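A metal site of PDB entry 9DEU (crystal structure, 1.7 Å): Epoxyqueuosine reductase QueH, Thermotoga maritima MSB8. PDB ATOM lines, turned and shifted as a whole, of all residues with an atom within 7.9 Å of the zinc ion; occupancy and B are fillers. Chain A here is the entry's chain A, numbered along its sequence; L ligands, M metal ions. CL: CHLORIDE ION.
The backbone NH (N) of Cys 9 sits at hydrogen-bond distance from the side-chain hydroxyl (OG1) of Thr 113, at 3.0 Å. NE2 of Gln 166 lies close to SG of Cys 10, at 3.2 Å.
Of the 21 residues printed, 3 come within 4 Å of the zinc ion.
The zinc ion is bound by the side-chain carboxylate of Asp 13, the side-chain sulfur of Cys 9, a chlorine (CL) of the ligand and the side-chain sulfur of Cys 10.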
ATOM      1  N   HIS A   7       0.432   7.565 -16.680  1.00  0.00           N
ATOM      2  CA  HIS A   7       0.503   8.562 -17.731  1.00  0.00           C
ATOM      3  C   HIS A   7       1.919   8.644 -18.285  1.00  0.00           C
ATOM      4  O   HIS A   7       2.899   8.602 -17.530  1.00  0.00           O
ATOM      5  CB  HIS A   7       0.052   9.925 -17.171  1.00  0.00           C
ATOM      6  CG  HIS A   7       0.415  11.082 -18.042  1.00  0.00           C
ATOM      7  ND1 HIS A   7       1.538  11.847 -17.817  1.00  0.00           N
ATOM      8  CD2 HIS A   7      -0.151  11.554 -19.184  1.00  0.00           C
ATOM      9  CE1 HIS A   7       1.660  12.735 -18.791  1.00  0.00           C
ATOM     10  NE2 HIS A   7       0.642  12.584 -19.626  1.00  0.00           N
ATOM     11  N   VAL A   8       2.031   8.739 -19.609  1.00  0.00           N
ATOM     12  CA  VAL A   8       3.330   8.885 -20.277  1.00  0.00           C
ATOM     13  C   VAL A   8       3.394  10.234 -20.958  1.00  0.00           C
ATOM     14  O   VAL A   8       2.567  10.515 -21.833  1.00  0.00           O
ATOM     15  CB  VAL A   8       3.585   7.787 -21.299  1.00  0.00           C
ATOM     16  CG1 VAL A   8       4.955   8.002 -22.025  1.00  0.00           C
ATOM     17  CG2 VAL A   8       3.598   6.466 -20.607  1.00  0.00           C
ATOM     18  N   CYS A   9       4.419  11.025 -20.625  1.00  0.00           N
ATOM     19  CA  CYS A   9       4.717  12.306 -21.270  1.00  0.00           C
ATOM     20  C   CYS A   9       5.606  12.173 -22.512  1.00  0.00           C
ATOM     21  O   CYS A   9       5.363  12.828 -23.526  1.00  0.00           O
ATOM     22  CB  CYS A   9       5.351  13.241 -20.247  1.00  0.00           C
ATOM     23  SG  CYS A   9       6.808  12.612 -19.362  1.00  0.00           S
ATOM     24  N   CYS A  10       6.628  11.303 -22.480  1.00  0.00           N
ATOM     25  CA  CYS A  10       7.574  11.169 -23.571  1.00  0.00           C
ATOM     26  C   CYS A  10       8.343   9.864 -23.394  1.00  0.00           C
ATOM     27  O   CYS A  10       8.392   9.295 -22.298  1.00  0.00           O
ATOM     28  CB  CYS A  10       8.570  12.341 -23.636  1.00  0.00           C
ATOM     29  SG  CYS A  10       9.697  12.413 -22.200  1.00  0.00           S
ATOM     30  N   ALA A  11       8.962   9.434 -24.488  1.00  0.00           N
ATOM     31  CA  ALA A  11       9.708   8.169 -24.458  1.00  0.00           C
ATOM     32  C   ALA A  11      10.914   8.209 -23.530  1.00  0.00           C
ATOM     33  O   ALA A  11      11.181   7.184 -22.853  1.00  0.00           O
ATOM     34  CB  ALA A  11      10.132   7.811 -25.891  1.00  0.00           C
ATOM     35  N   PRO A  12      11.731   9.258 -23.495  1.00  0.00           N
ATOM     36  CA  PRO A  12      12.866   9.246 -22.557  1.00  0.00           C
ATOM     37  C   PRO A  12      12.442   9.085 -21.107  1.00  0.00           C
ATOM     38  O   PRO A  12      13.079   8.328 -20.370  1.00  0.00           O
ATOM     39  CB  PRO A  12      13.549  10.598 -22.800  1.00  0.00           C
ATOM     40  CG  PRO A  12      13.199  10.941 -24.218  1.00  0.00           C
ATOM     41  CD  PRO A  12      11.754  10.472 -24.351  1.00  0.00           C
ATOM     42  N   ASP A  13      11.356   9.743 -20.694  1.00  0.00           N
ATOM     43  CA  ASP A  13      10.917   9.567 -19.319  1.00  0.00           C
ATOM     44  C   ASP A  13      10.264   8.209 -19.098  1.00  0.00           C
ATOM     45  O   ASP A  13      10.329   7.661 -17.994  1.00  0.00           O
ATOM     46  CB  ASP A  13       9.994  10.712 -18.908  1.00  0.00           C
ATOM     47  CG  ASP A  13      10.736  12.066 -18.868  1.00  0.00           C
ATOM     48  OD1 ASP A  13      11.951  12.060 -18.557  1.00  0.00           O
ATOM     49  OD2 ASP A  13      10.105  13.095 -19.178  1.00  0.00           O
ATOM     50  N   LEU A  14       9.622   7.640 -20.143  1.00  0.00           N
ATOM     51  CA  LEU A  14       9.136   6.251 -20.060  1.00  0.00           C
ATOM     52  C   LEU A  14      10.311   5.286 -19.836  1.00  0.00           C
ATOM     53  O   LEU A  14      10.211   4.354 -19.034  1.00  0.00           O
ATOM     54  CB  LEU A  14       8.375   5.884 -21.349  1.00  0.00           C
ATOM     55  CG  LEU A  14       7.881   4.433 -21.477  1.00  0.00           C
ATOM     56  CD1 LEU A  14       6.932   4.076 -20.339  1.00  0.00           C
ATOM     57  CD2 LEU A  14       7.174   4.293 -22.870  1.00  0.00           C
ATOM     58  N   ASN A  30      -1.519  13.654 -24.088  1.00  0.00           N
ATOM     59  CA  ASN A  30      -0.802  14.911 -23.993  1.00  0.00           C
ATOM     60  C   ASN A  30      -1.327  15.929 -24.992  1.00  0.00           C
ATOM     61  O   ASN A  30      -0.598  16.305 -25.927  1.00  0.00           O
ATOM     62  CB  ASN A  30       0.692  14.717 -24.253  1.00  0.00           C
ATOM     63  CG  ASN A  30       1.366  13.775 -23.243  1.00  0.00           C
ATOM     64  OD1 ASN A  30       1.660  14.180 -22.133  1.00  0.00           O
ATOM     65  ND2 ASN A  30       1.587  12.512 -23.635  1.00  0.00           N
ATOM     66  N   ARG A  42       6.494  12.578 -30.941  1.00  0.00           N
ATOM     67  CA  ARG A  42       6.650  12.063 -29.580  1.00  0.00           C
ATOM     68  C   ARG A  42       5.909  10.755 -29.405  1.00  0.00           C
ATOM     69  O   ARG A  42       6.420   9.824 -28.763  1.00  0.00           O
ATOM     70  CB  ARG A  42       6.168  13.106 -28.585  1.00  0.00           C
ATOM     71  CG  ARG A  42       7.132  14.262 -28.592  1.00  0.00           C
ATOM     72  CD  ARG A  42       7.077  15.111 -27.347  1.00  0.00           C
ATOM     73  NE  ARG A  42       7.643  16.423 -27.610  1.00  0.00           N
ATOM     74  CZ  ARG A  42       7.675  17.412 -26.727  1.00  0.00           C
ATOM     75  NH1 ARG A  42       7.194  17.263 -25.504  1.00  0.00           N
ATOM     76  NH2 ARG A  42       8.199  18.582 -27.097  1.00  0.00           N
ATOM     77  N   THR A 112       2.597   8.839 -13.110  1.00  0.00           N
ATOM     78  CA  THR A 112       2.986   9.519 -14.335  1.00  0.00           C
ATOM     79  C   THR A 112       4.495   9.440 -14.509  1.00  0.00           C
ATOM     80  O   THR A 112       5.231   9.493 -13.525  1.00  0.00           O
ATOM     81  CB  THR A 112       2.547  10.991 -14.337  1.00  0.00           C
ATOM     82  OG1 THR A 112       3.123  11.647 -15.477  1.00  0.00           O
ATOM     83  CG2 THR A 112       3.012  11.721 -13.078  1.00  0.00           C
ATOM     84  N   THR A 113       4.947   9.325 -15.772  1.00  0.00           N
ATOM     85  CA  THR A 113       6.394   9.394 -16.046  1.00  0.00           C
ATOM     86  C   THR A 113       6.953  10.804 -15.874  1.00  0.00           C
ATOM     87  O   THR A 113       8.180  10.989 -15.949  1.00  0.00           O
ATOM     88  CB  THR A 113       6.718   8.886 -17.472  1.00  0.00           C
ATOM     89  OG1 THR A 113       6.091   9.721 -18.449  1.00  0.00           O
ATOM     90  CG2 THR A 113       6.226   7.441 -17.668  1.00  0.00           C
ATOM     91  N   LEU A 114       6.113  11.812 -15.643  1.00  0.00           N
ATOM     92  CA  LEU A 114       6.655  13.128 -15.321  1.00  0.00           C
ATOM     93  C   LEU A 114       7.467  13.062 -14.047  1.00  0.00           C
ATOM     94  O   LEU A 114       8.336  13.908 -13.824  1.00  0.00           O
ATOM     95  CB  LEU A 114       5.535  14.163 -15.164  1.00  0.00           C
ATOM     96  CG  LEU A 114       4.751  14.552 -16.399  1.00  0.00           C
ATOM     97  CD1 LEU A 114       3.442  15.175 -15.944  1.00  0.00           C
ATOM     98  CD2 LEU A 114       5.558  15.523 -17.243  1.00  0.00           C
ATOM     99  N   LEU A 115       7.201  12.064 -13.199  1.00  0.00           N
ATOM    100  CA  LEU A 115       8.019  11.886 -11.992  1.00  0.00           C
ATOM    101  C   LEU A 115       9.459  11.536 -12.318  1.00  0.00           C
ATOM    102  O   LEU A 115      10.321  11.624 -11.438  1.00  0.00           O
ATOM    103  CB  LEU A 115       7.438  10.786 -11.132  1.00  0.00           C
ATOM    104  CG  LEU A 115       6.101  11.101 -10.472  1.00  0.00           C
ATOM    105  CD1 LEU A 115       5.575   9.837  -9.814  1.00  0.00           C
ATOM    106  CD2 LEU A 115       6.302  12.205  -9.407  1.00  0.00           C
ATOM    107  N   ALA A 116       9.721  11.122 -13.547  1.00  0.00           N
ATOM    108  CA  ALA A 116      11.068  10.813 -13.982  1.00  0.00           C
ATOM    109  C   ALA A 116      11.746  11.994 -14.641  1.00  0.00           C
ATOM    110  O   ALA A 116      12.909  11.899 -15.028  1.00  0.00           O
ATOM    111  CB  ALA A 116      11.037   9.627 -14.968  1.00  0.00           C
ATOM    112  N   SER A 117      11.388  12.777 -14.695  1.00  0.00           N
ATOM    113  CA  SER A 117      11.716  13.919 -15.532  1.00  0.00           C
ATOM    114  C   SER A 117      12.553  14.902 -14.728  1.00  0.00           C
ATOM    115  O   SER A 117      12.098  15.365 -13.687  1.00  0.00           O
ATOM    116  CB  SER A 117      10.443  14.590 -16.035  1.00  0.00           C
ATOM    117  OG  SER A 117      10.735  15.738 -16.813  1.00  0.00           O
ATOM    118  N   PRO A 118      13.784  15.168 -15.205  1.00  0.00           N
ATOM    119  CA  PRO A 118      14.762  15.893 -14.370  1.00  0.00           C
ATOM    120  C   PRO A 118      14.386  17.341 -14.106  1.00  0.00           C
ATOM    121  O   PRO A 118      14.755  17.891 -13.059  1.00  0.00           O
ATOM    122  CB  PRO A 118      16.059  15.784 -15.184  1.00  0.00           C
ATOM    123  CG  PRO A 118      15.844  14.623 -16.102  1.00  0.00           C
ATOM    124  CD  PRO A 118      14.390  14.633 -16.440  1.00  0.00           C
ATOM    125  N   LYS A 120      11.326  18.595 -13.668  1.00  0.00           N
ATOM    126  CA  LYS A 120      10.034  18.870 -13.065  1.00  0.00           C
ATOM    127  C   LYS A 120      10.163  18.986 -11.544  1.00  0.00           C
ATOM    128  O   LYS A 120      11.179  18.664 -10.923  1.00  0.00           O
ATOM    129  CB  LYS A 120       9.023  17.792 -13.449  1.00  0.00           C
ATOM    130  CG  LYS A 120       8.644  17.751 -14.942  1.00  0.00           C
ATOM    131  CD  LYS A 120       8.215  19.115 -15.480  1.00  0.00           C
ATOM    132  CE  LYS A 120       8.094  19.106 -17.000  1.00  0.00           C
ATOM    133  NZ  LYS A 120       9.200  18.332 -17.662  1.00  0.00           N
ATOM    134  N   GLN A 166      13.524  15.294 -26.821  1.00  0.00           N
ATOM    135  CA  GLN A 166      13.061  16.641 -27.126  1.00  0.00           C
ATOM    136  C   GLN A 166      13.712  17.678 -26.226  1.00  0.00           C
ATOM    137  O   GLN A 166      14.223  17.388 -25.143  1.00  0.00           O
ATOM    138  CB  GLN A 166      11.532  16.726 -27.027  1.00  0.00           C
ATOM    139  CG  GLN A 166      10.986  16.631 -25.617  1.00  0.00           C
ATOM    140  CD  GLN A 166      11.027  15.213 -25.069  1.00  0.00           C
ATOM    141  OE1 GLN A 166      11.462  14.298 -25.745  1.00  0.00           O
ATOM    142  NE2 GLN A 166      10.563  15.032 -23.846  1.00  0.00           N
ATOM    143  N   TYR A 168      12.042  20.762 -25.748  1.00  0.00           N
ATOM    144  CA  TYR A 168      11.134  21.615 -24.991  1.00  0.00           C
ATOM    145  C   TYR A 168       9.981  20.778 -24.450  1.00  0.00           C
ATOM    146  O   TYR A 168       9.775  19.625 -24.859  1.00  0.00           O
ATOM    147  CB  TYR A 168      10.614  22.786 -25.832  1.00  0.00           C
ATOM    148  CG  TYR A 168       9.647  22.407 -26.940  1.00  0.00           C
ATOM    149  CD1 TYR A 168      10.091  21.797 -28.111  1.00  0.00           C
ATOM    150  CD2 TYR A 168       8.296  22.683 -26.818  1.00  0.00           C
ATOM    151  CE1 TYR A 168       9.208  21.455 -29.123  1.00  0.00           C
ATOM    152  CE2 TYR A 168       7.403  22.351 -27.809  1.00  0.00           C
ATOM    153  CZ  TYR A 168       7.856  21.746 -28.968  1.00  0.00           C
ATOM    154  OH  TYR A 168       6.931  21.433 -29.941  1.00  0.00           O
ATOM    155  N   CYS A 169       9.219  21.371 -23.523  1.00  0.00           N
ATOM    156  CA  CYS A 169       8.223  20.629 -22.752  1.00  0.00           C
ATOM    157  C   CYS A 169       7.079  20.130 -23.630  1.00  0.00           C
ATOM    158  O   CYS A 169       6.600  19.003 -23.433  1.00  0.00           O
ATOM    159  CB  CYS A 169       7.685  21.512 -21.625  1.00  0.00           C
ATOM    160  SG  CYS A 169       6.995  20.608 -20.204  1.00  0.00           S
HETATM  161 CL    CL L   1       8.337  15.607 -20.763  1.00  0.00          CL
HETATM  162 ZN    ZN M   1       8.629  13.398 -20.424  1.00  0.00          ZN
